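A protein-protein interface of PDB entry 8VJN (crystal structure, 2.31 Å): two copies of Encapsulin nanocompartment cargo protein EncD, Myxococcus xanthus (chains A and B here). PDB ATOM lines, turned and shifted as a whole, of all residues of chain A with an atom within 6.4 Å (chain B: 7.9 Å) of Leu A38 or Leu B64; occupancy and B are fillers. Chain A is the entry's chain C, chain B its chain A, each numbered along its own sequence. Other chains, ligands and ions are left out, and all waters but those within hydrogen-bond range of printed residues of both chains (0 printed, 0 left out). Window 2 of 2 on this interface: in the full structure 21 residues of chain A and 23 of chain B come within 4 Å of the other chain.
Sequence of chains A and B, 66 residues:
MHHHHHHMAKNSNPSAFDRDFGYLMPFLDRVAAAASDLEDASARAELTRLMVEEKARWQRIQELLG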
ATOM      1  N   VAL A  31     -22.815  -2.634  21.815  1.00  0.00           N
ATOM      2  CA  VAL A  31     -21.790  -3.300  20.998  1.00  0.00           C
ATOM      3  C   VAL A  31     -22.039  -3.053  19.509  1.00  0.00           C
ATOM      4  O   VAL A  31     -21.104  -2.776  18.742  1.00  0.00           O
ATOM      5  CB  VAL A  31     -21.723  -4.806  21.337  1.00  0.00           C
ATOM      6  CG1 VAL A  31     -20.775  -5.562  20.400  1.00  0.00           C
ATOM      7  CG2 VAL A  31     -21.251  -4.974  22.780  1.00  0.00           C
ATOM      8  N   ALA A  34     -20.822   0.444  18.970  1.00  0.00           N
ATOM      9  CA  ALA A  34     -19.366   0.506  18.947  1.00  0.00           C
ATOM     10  C   ALA A  34     -18.781  -0.097  17.679  1.00  0.00           C
ATOM     11  O   ALA A  34     -17.642   0.234  17.331  1.00  0.00           O
ATOM     12  CB  ALA A  34     -18.783  -0.207  20.164  1.00  0.00           C
ATOM     13  N   ALA A  35     -19.534  -0.973  16.996  1.00  0.00           N
ATOM     14  CA  ALA A  35     -19.091  -1.529  15.715  1.00  0.00           C
ATOM     15  C   ALA A  35     -18.746  -0.441  14.704  1.00  0.00           C
ATOM     16  O   ALA A  35     -17.772  -0.577  13.956  1.00  0.00           O
ATOM     17  CB  ALA A  35     -20.163  -2.462  15.142  1.00  0.00           C
ATOM     18  N   SER A  36     -19.509   0.665  14.692  1.00  0.00           N
ATOM     19  CA  SER A  36     -19.223   1.775  13.777  1.00  0.00           C
ATOM     20  C   SER A  36     -17.913   2.475  14.113  1.00  0.00           C
ATOM     21  O   SER A  36     -17.289   3.082  13.233  1.00  0.00           O
ATOM     22  CB  SER A  36     -20.361   2.802  13.798  1.00  0.00           C
ATOM     23  OG  SER A  36     -21.468   2.346  13.041  1.00  0.00           O
ATOM     24  N   ASP A  37     -17.478   2.400  15.366  1.00  0.00           N
ATOM     25  CA  ASP A  37     -16.350   3.187  15.840  1.00  0.00           C
ATOM     26  C   ASP A  37     -15.000   2.526  15.597  1.00  0.00           C
ATOM     27  O   ASP A  37     -13.974   3.150  15.896  1.00  0.00           O
ATOM     28  CB  ASP A  37     -16.503   3.486  17.342  1.00  0.00           C
ATOM     29  CG  ASP A  37     -17.499   4.606  17.618  1.00  0.00           C
ATOM     30  OD1 ASP A  37     -17.284   5.727  17.115  1.00  0.00           O
ATOM     31  OD2 ASP A  37     -18.499   4.370  18.327  1.00  0.00           O
ATOM     32  N   LEU A  38     -14.961   1.287  15.091  1.00  0.00           N
ATOM     33  CA  LEU A  38     -13.672   0.655  14.819  1.00  0.00           C
ATOM     34  C   LEU A  38     -13.032   1.310  13.601  1.00  0.00           C
ATOM     35  O   LEU A  38     -13.688   1.512  12.571  1.00  0.00           O
ATOM     36  CB  LEU A  38     -13.811  -0.857  14.601  1.00  0.00           C
ATOM     37  CG  LEU A  38     -14.055  -1.839  15.757  1.00  0.00           C
ATOM     38  CD1 LEU A  38     -13.323  -1.393  17.011  1.00  0.00           C
ATOM     39  CD2 LEU A  38     -15.523  -2.043  16.033  1.00  0.00           C
ATOM     40  N   GLU A  39     -11.756   1.677  13.736  1.00  0.00           N
ATOM     41  CA  GLU A  39     -11.034   2.241  12.601  1.00  0.00           C
ATOM     42  C   GLU A  39     -10.793   1.188  11.527  1.00  0.00           C
ATOM     43  O   GLU A  39     -10.920   1.482  10.334  1.00  0.00           O
ATOM     44  CB  GLU A  39      -9.717   2.867  13.072  1.00  0.00           C
ATOM     45  CG  GLU A  39      -9.909   3.993  14.084  1.00  0.00           C
ATOM     46  CD  GLU A  39      -8.743   4.137  15.033  1.00  0.00           C
ATOM     47  OE1 GLU A  39      -7.793   3.328  14.923  1.00  0.00           O
ATOM     48  OE2 GLU A  39      -8.781   5.061  15.879  1.00  0.00           O
ATOM     49  N   ASP A  40     -10.499  -0.046  11.930  1.00  0.00           N
ATOM     50  CA  ASP A  40     -10.245  -1.129  10.994  1.00  0.00           C
ATOM     51  C   ASP A  40     -11.528  -1.539  10.265  1.00  0.00           C
ATOM     52  O   ASP A  40     -12.557  -1.805  10.899  1.00  0.00           O
ATOM     53  CB  ASP A  40      -9.631  -2.307  11.747  1.00  0.00           C
ATOM     54  CG  ASP A  40      -9.309  -3.479  10.841  1.00  0.00           C
ATOM     55  OD1 ASP A  40      -9.063  -3.243   9.637  1.00  0.00           O
ATOM     56  OD2 ASP A  40      -9.275  -4.627  11.340  1.00  0.00           O
ATOM     57  N   ALA A  41     -11.450  -1.606   8.930  1.00  0.00           N
ATOM     58  CA  ALA A  41     -12.622  -1.888   8.100  1.00  0.00           C
ATOM     59  C   ALA A  41     -13.062  -3.342   8.205  1.00  0.00           C
ATOM     60  O   ALA A  41     -14.268  -3.634   8.192  1.00  0.00           O
ATOM     61  CB  ALA A  41     -12.324  -1.545   6.645  1.00  0.00           C
ATOM     62  N   SER A  42     -12.107  -4.267   8.280  1.00  0.00           N
ATOM     63  CA  SER A  42     -12.445  -5.674   8.464  1.00  0.00           C
ATOM     64  C   SER A  42     -13.117  -5.914   9.810  1.00  0.00           C
ATOM     65  O   SER A  42     -14.138  -6.610   9.885  1.00  0.00           O
ATOM     66  CB  SER A  42     -11.193  -6.535   8.340  1.00  0.00           C
ATOM     67  OG  SER A  42     -10.826  -6.679   6.980  1.00  0.00           O
ATOM     68  N   ALA A  43     -12.540  -5.368  10.887  1.00  0.00           N
ATOM     69  CA  ALA A  43     -13.140  -5.510  12.209  1.00  0.00           C
ATOM     70  C   ALA A  43     -14.540  -4.914  12.248  1.00  0.00           C
ATOM     71  O   ALA A  43     -15.465  -5.527  12.788  1.00  0.00           O
ATOM     72  CB  ALA A  43     -12.247  -4.856  13.267  1.00  0.00           C
ATOM     73  N   ARG A  44     -14.717  -3.734  11.657  1.00  0.00           N
ATOM     74  CA  ARG A  44     -16.038  -3.107  11.600  1.00  0.00           C
ATOM     75  C   ARG A  44     -17.053  -3.975  10.848  1.00  0.00           C
ATOM     76  O   ARG A  44     -18.180  -4.169  11.326  1.00  0.00           O
ATOM     77  CB  ARG A  44     -15.913  -1.724  10.945  1.00  0.00           C
ATOM     78  CG  ARG A  44     -17.244  -0.995  10.686  1.00  0.00           C
ATOM     79  CD  ARG A  44     -17.008   0.364  10.019  1.00  0.00           C
ATOM     80  NE  ARG A  44     -15.607   0.761  10.113  1.00  0.00           N
ATOM     81  CZ  ARG A  44     -14.809   0.990   9.074  1.00  0.00           C
ATOM     82  NH1 ARG A  44     -15.253   0.924   7.828  1.00  0.00           N
ATOM     83  NH2 ARG A  44     -13.531   1.290   9.293  1.00  0.00           N
ATOM     84  N   GLU A  46     -16.907  -7.308  10.323  1.00  0.00           N
ATOM     85  CA  GLU A  46     -17.170  -8.541  11.052  1.00  0.00           C
ATOM     86  C   GLU A  46     -18.074  -8.285  12.246  1.00  0.00           C
ATOM     87  O   GLU A  46     -19.058  -8.999  12.444  1.00  0.00           O
ATOM     88  CB  GLU A  46     -15.871  -9.184  11.513  1.00  0.00           C
ATOM     89  CG  GLU A  46     -16.069 -10.561  12.114  1.00  0.00           C
ATOM     90  CD  GLU A  46     -14.762 -11.145  12.604  1.00  0.00           C
ATOM     91  OE1 GLU A  46     -13.705 -10.586  12.213  1.00  0.00           O
ATOM     92  OE2 GLU A  46     -14.781 -12.131  13.389  1.00  0.00           O
ATOM     93  N   LEU A  47     -17.771  -7.259  13.041  1.00  0.00           N
ATOM     94  CA  LEU A  47     -18.595  -7.009  14.208  1.00  0.00           C
ATOM     95  C   LEU A  47     -20.002  -6.589  13.812  1.00  0.00           C
ATOM     96  O   LEU A  47     -20.970  -7.016  14.449  1.00  0.00           O
ATOM     97  CB  LEU A  47     -17.926  -5.972  15.092  1.00  0.00           C
ATOM     98  CG  LEU A  47     -18.542  -5.764  16.473  1.00  0.00           C
ATOM     99  CD1 LEU A  47     -18.862  -7.092  17.152  1.00  0.00           C
ATOM    100  CD2 LEU A  47     -17.607  -4.916  17.306  1.00  0.00           C
ATOM    101  N   LEU A  50     -21.788  -9.695  12.874  1.00  0.00           N
ATOM    102  CA  LEU A  50     -21.989 -10.501  14.071  1.00  0.00           C
ATOM    103  C   LEU A  50     -23.131  -9.954  14.928  1.00  0.00           C
ATOM    104  O   LEU A  50     -23.956 -10.717  15.432  1.00  0.00           O
ATOM    105  CB  LEU A  50     -20.687 -10.570  14.863  1.00  0.00           C
ATOM    106  CG  LEU A  50     -19.666 -11.570  14.304  1.00  0.00           C
ATOM    107  CD1 LEU A  50     -18.369 -11.403  15.025  1.00  0.00           C
ATOM    108  CD2 LEU A  50     -20.144 -12.994  14.434  1.00  0.00           C
ATOM    109  N   SER B  15     -11.392  -0.418  27.151  1.00  0.00           N
ATOM    110  CA  SER B  15     -12.708  -0.927  26.691  1.00  0.00           C
ATOM    111  C   SER B  15     -13.771  -0.588  27.725  1.00  0.00           C
ATOM    112  O   SER B  15     -13.538  -0.840  28.917  1.00  0.00           O
ATOM    113  CB  SER B  15     -12.681  -2.408  26.430  1.00  0.00           C
ATOM    114  OG  SER B  15     -12.229  -2.679  25.112  1.00  0.00           O
ATOM    115  N   PHE B  21     -18.259  -7.861  29.968  1.00  0.00           N
ATOM    116  CA  PHE B  21     -17.881  -9.242  29.666  1.00  0.00           C
ATOM    117  C   PHE B  21     -17.651 -10.047  30.932  1.00  0.00           C
ATOM    118  O   PHE B  21     -17.962 -11.258  30.965  1.00  0.00           O
ATOM    119  CB  PHE B  21     -16.643  -9.274  28.780  1.00  0.00           C
ATOM    120  CG  PHE B  21     -16.951  -9.061  27.334  1.00  0.00           C
ATOM    121  CD1 PHE B  21     -17.546 -10.064  26.596  1.00  0.00           C
ATOM    122  CD2 PHE B  21     -16.671  -7.857  26.722  1.00  0.00           C
ATOM    123  CE1 PHE B  21     -17.845  -9.886  25.265  1.00  0.00           C
ATOM    124  CE2 PHE B  21     -16.974  -7.662  25.375  1.00  0.00           C
ATOM    125  CZ  PHE B  21     -17.557  -8.675  24.648  1.00  0.00           C
ATOM    126  N   ARG B  57     -18.574 -17.139  19.974  1.00  0.00           N
ATOM    127  CA  ARG B  57     -18.803 -15.878  19.292  1.00  0.00           C
ATOM    128  C   ARG B  57     -18.513 -14.686  20.192  1.00  0.00           C
ATOM    129  O   ARG B  57     -17.880 -13.722  19.746  1.00  0.00           O
ATOM    130  CB  ARG B  57     -20.232 -15.842  18.782  1.00  0.00           C
ATOM    131  CG  ARG B  57     -20.388 -16.757  17.570  1.00  0.00           C
ATOM    132  CD  ARG B  57     -21.768 -17.315  17.461  1.00  0.00           C
ATOM    133  NE  ARG B  57     -22.667 -16.227  17.148  1.00  0.00           N
ATOM    134  CZ  ARG B  57     -22.891 -15.812  15.915  1.00  0.00           C
ATOM    135  NH1 ARG B  57     -22.345 -16.424  14.877  1.00  0.00           N
ATOM    136  NH2 ARG B  57     -23.677 -14.756  15.722  1.00  0.00           N
ATOM    137  N   TRP B  58     -18.933 -14.720  21.457  1.00  0.00           N
ATOM    138  CA  TRP B  58     -18.619 -13.562  22.297  1.00  0.00           C
ATOM    139  C   TRP B  58     -17.138 -13.476  22.645  1.00  0.00           C
ATOM    140  O   TRP B  58     -16.643 -12.356  22.825  1.00  0.00           O
ATOM    141  CB  TRP B  58     -19.480 -13.538  23.558  1.00  0.00           C
ATOM    142  CG  TRP B  58     -20.803 -12.979  23.175  1.00  0.00           C
ATOM    143  CD1 TRP B  58     -21.940 -13.683  22.910  1.00  0.00           C
ATOM    144  CD2 TRP B  58     -21.095 -11.612  22.883  1.00  0.00           C
ATOM    145  NE1 TRP B  58     -22.936 -12.830  22.505  1.00  0.00           N
ATOM    146  CE2 TRP B  58     -22.441 -11.549  22.489  1.00  0.00           C
ATOM    147  CE3 TRP B  58     -20.353 -10.423  22.949  1.00  0.00           C
ATOM    148  CZ2 TRP B  58     -23.065 -10.352  22.155  1.00  0.00           C
ATOM    149  CZ3 TRP B  58     -20.965  -9.247  22.620  1.00  0.00           C
ATOM    150  CH2 TRP B  58     -22.317  -9.212  22.227  1.00  0.00           C
ATOM    151  N   GLN B  59     -16.403 -14.613  22.690  1.00  0.00           N
ATOM    152  CA  GLN B  59     -14.942 -14.522  22.807  1.00  0.00           C
ATOM    153  C   GLN B  59     -14.335 -13.813  21.608  1.00  0.00           C
ATOM    154  O   GLN B  59     -13.422 -12.979  21.762  1.00  0.00           O
ATOM    155  CB  GLN B  59     -14.287 -15.885  22.939  1.00  0.00           C
ATOM    156  CG  GLN B  59     -14.519 -16.642  24.222  1.00  0.00           C
ATOM    157  CD  GLN B  59     -14.137 -18.103  24.051  1.00  0.00           C
ATOM    158  OE1 GLN B  59     -13.176 -18.433  23.350  1.00  0.00           O
ATOM    159  NE2 GLN B  59     -14.873 -18.992  24.745  1.00  0.00           N
ATOM    160  N   ARG B  60     -14.843 -14.119  20.401  1.00  0.00           N
ATOM    161  CA  ARG B  60     -14.433 -13.375  19.205  1.00  0.00           C
ATOM    162  C   ARG B  60     -14.795 -11.890  19.304  1.00  0.00           C
ATOM    163  O   ARG B  60     -13.971 -11.028  18.989  1.00  0.00           O
ATOM    164  CB  ARG B  60     -15.073 -13.975  17.955  1.00  0.00           C
ATOM    165  CG  ARG B  60     -14.701 -13.289  16.600  1.00  0.00           C
ATOM    166  CD  ARG B  60     -13.275 -12.662  16.499  1.00  0.00           C
ATOM    167  NE  ARG B  60     -12.746 -12.606  15.141  1.00  0.00           N
ATOM    168  CZ  ARG B  60     -11.558 -12.106  14.820  1.00  0.00           C
ATOM    169  NH1 ARG B  60     -10.743 -11.621  15.744  1.00  0.00           N
ATOM    170  NH2 ARG B  60     -11.176 -12.099  13.540  1.00  0.00           N
ATOM    171  N   ILE B  61     -16.044 -11.572  19.646  1.00  0.00           N
ATOM    172  CA  ILE B  61     -16.468 -10.171  19.709  1.00  0.00           C
ATOM    173  C   ILE B  61     -15.588  -9.407  20.691  1.00  0.00           C
ATOM    174  O   ILE B  61     -15.162  -8.277  20.416  1.00  0.00           O
ATOM    175  CB  ILE B  61     -17.953 -10.065  20.096  1.00  0.00           C
ATOM    176  CG1 ILE B  61     -18.856 -10.493  18.938  1.00  0.00           C
ATOM    177  CG2 ILE B  61     -18.287  -8.636  20.469  1.00  0.00           C
ATOM    178  CD1 ILE B  61     -20.226 -10.959  19.363  1.00  0.00           C
ATOM    179  N   GLN B  62     -15.230 -10.055  21.808  1.00  0.00           N
ATOM    180  CA  GLN B  62     -14.343  -9.422  22.772  1.00  0.00           C
ATOM    181  C   GLN B  62     -12.970  -9.162  22.147  1.00  0.00           C
ATOM    182  O   GLN B  62     -12.368  -8.102  22.379  1.00  0.00           O
ATOM    183  CB  GLN B  62     -14.235 -10.281  24.039  1.00  0.00           C
ATOM    184  CG  GLN B  62     -13.103  -9.828  24.979  1.00  0.00           C
ATOM    185  CD  GLN B  62     -13.378 -10.046  26.456  1.00  0.00           C
ATOM    186  OE1 GLN B  62     -13.456 -11.183  26.924  1.00  0.00           O
ATOM    187  NE2 GLN B  62     -13.545  -8.947  27.200  1.00  0.00           N
ATOM    188  N   GLU B  63     -12.496 -10.075  21.284  1.00  0.00           N
ATOM    189  CA  GLU B  63     -11.296  -9.771  20.488  1.00  0.00           C
ATOM    190  C   GLU B  63     -11.489  -8.559  19.569  1.00  0.00           C
ATOM    191  O   GLU B  63     -10.587  -7.722  19.455  1.00  0.00           O
ATOM    192  CB  GLU B  63     -10.852 -10.985  19.654  1.00  0.00           C
ATOM    193  CG  GLU B  63      -9.840 -11.899  20.325  1.00  0.00           C
ATOM    194  CD  GLU B  63      -9.746 -13.280  19.669  1.00  0.00           C
ATOM    195  OE1 GLU B  63     -10.128 -13.405  18.474  1.00  0.00           O
ATOM    196  OE2 GLU B  63      -9.275 -14.236  20.353  1.00  0.00           O
ATOM    197  N   LEU B  64     -12.629  -8.476  18.866  1.00  0.00           N
ATOM    198  CA  LEU B  64     -12.834  -7.365  17.931  1.00  0.00           C
ATOM    199  C   LEU B  64     -12.961  -6.026  18.658  1.00  0.00           C
ATOM    200  O   LEU B  64     -12.655  -4.974  18.080  1.00  0.00           O
ATOM    201  CB  LEU B  64     -14.067  -7.579  17.039  1.00  0.00           C
ATOM    202  CG  LEU B  64     -14.149  -8.803  16.110  1.00  0.00           C
ATOM    203  CD1 LEU B  64     -15.578  -9.212  15.812  1.00  0.00           C
ATOM    204  CD2 LEU B  64     -13.406  -8.521  14.835  1.00  0.00           C
ATOM    205  N   LEU B  65     -13.399  -6.037  19.918  1.00  0.00           N
ATOM    206  CA  LEU B  65     -13.569  -4.775  20.626  1.00  0.00           C
ATOM    207  C   LEU B  65     -12.257  -4.254  21.199  1.00  0.00           C
ATOM    208  O   LEU B  65     -12.113  -3.043  21.393  1.00  0.00           O
ATOM    209  CB  LEU B  65     -14.614  -4.928  21.739  1.00  0.00           C
ATOM    210  CG  LEU B  65     -16.040  -5.037  21.204  1.00  0.00           C
ATOM    211  CD1 LEU B  65     -17.017  -5.524  22.276  1.00  0.00           C
ATOM    212  CD2 LEU B  65     -16.485  -3.718  20.589  1.00  0.00           C
ATOM    213  N   GLY B  66     -11.299  -5.134  21.476  1.00  0.00           N
ATOM    214  CA  GLY B  66     -10.028  -4.710  22.046  1.00  0.00           C
ATOM    215  C   GLY B  66      -9.177  -3.838  21.132  1.00  0.00           C
ATOM    216  O   GLY B  66      -8.818  -4.216  20.009  1.00  0.00           O
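The guanidinium group of Arg B60 is in salt-bridge range of the side-chain carboxylate of Glu A46 (2.7 Å).
Of the printed residues of chain B, Val A31 touches Ile B61. Printed residues of chain B within 4 Å of Leu A38: Leu B64. Printed residues of chain B within 4 Å of Glu A46: Arg B60 and Leu B64. Of the printed residues of chain A, Leu B64 touches Leu A38, Glu A46 and Leu A50. Printed residues of chain A within 4 Å of Leu B65: Leu A47 (3.7 Å). The nearest printed residue of chain A that does not touch Leu B64 is Ala A43 (4.004 Å). The nearest printed residue of chain B that does not touch Leu A47 is Leu B64 (4.04 Å).
Printed residues of chain A that touch a printed residue of chain B: Val A31, Leu A38, Glu A46, Leu A47 and Leu A50. Hydrophobic or aromatic side chains of chain A that line the printed part of chain B: Val A31, Leu A38, Leu A47 and Leu A50. Among the printed residues, Asp or Glu carboxylates within 4 Å of a Lys or Arg side-chain nitrogen of the other chain: Glu A46 with Arg B60.
Among the printed residues, merely in contact across the chains: Glu A46 with Leu B64 (3.4 Å), Leu A50 with Leu B64 (3.6 Å), Leu A47 with Leu B65 (3.7 Å), Leu A47 with Ile B61 (3.7 Å), Leu A38 with Leu B64 (3.8 Å) and Val A31 with Ile B61 (3.96 Å).
O of Leu A38 sits at hydrogen-bond distance from NE of Arg A44. The guanidinium group (NH1) of Arg B60 lies within salt-bridge range of the side-chain carboxylate (OE1) of Glu B63 (3.3 Å).
No position is printed for both chains.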
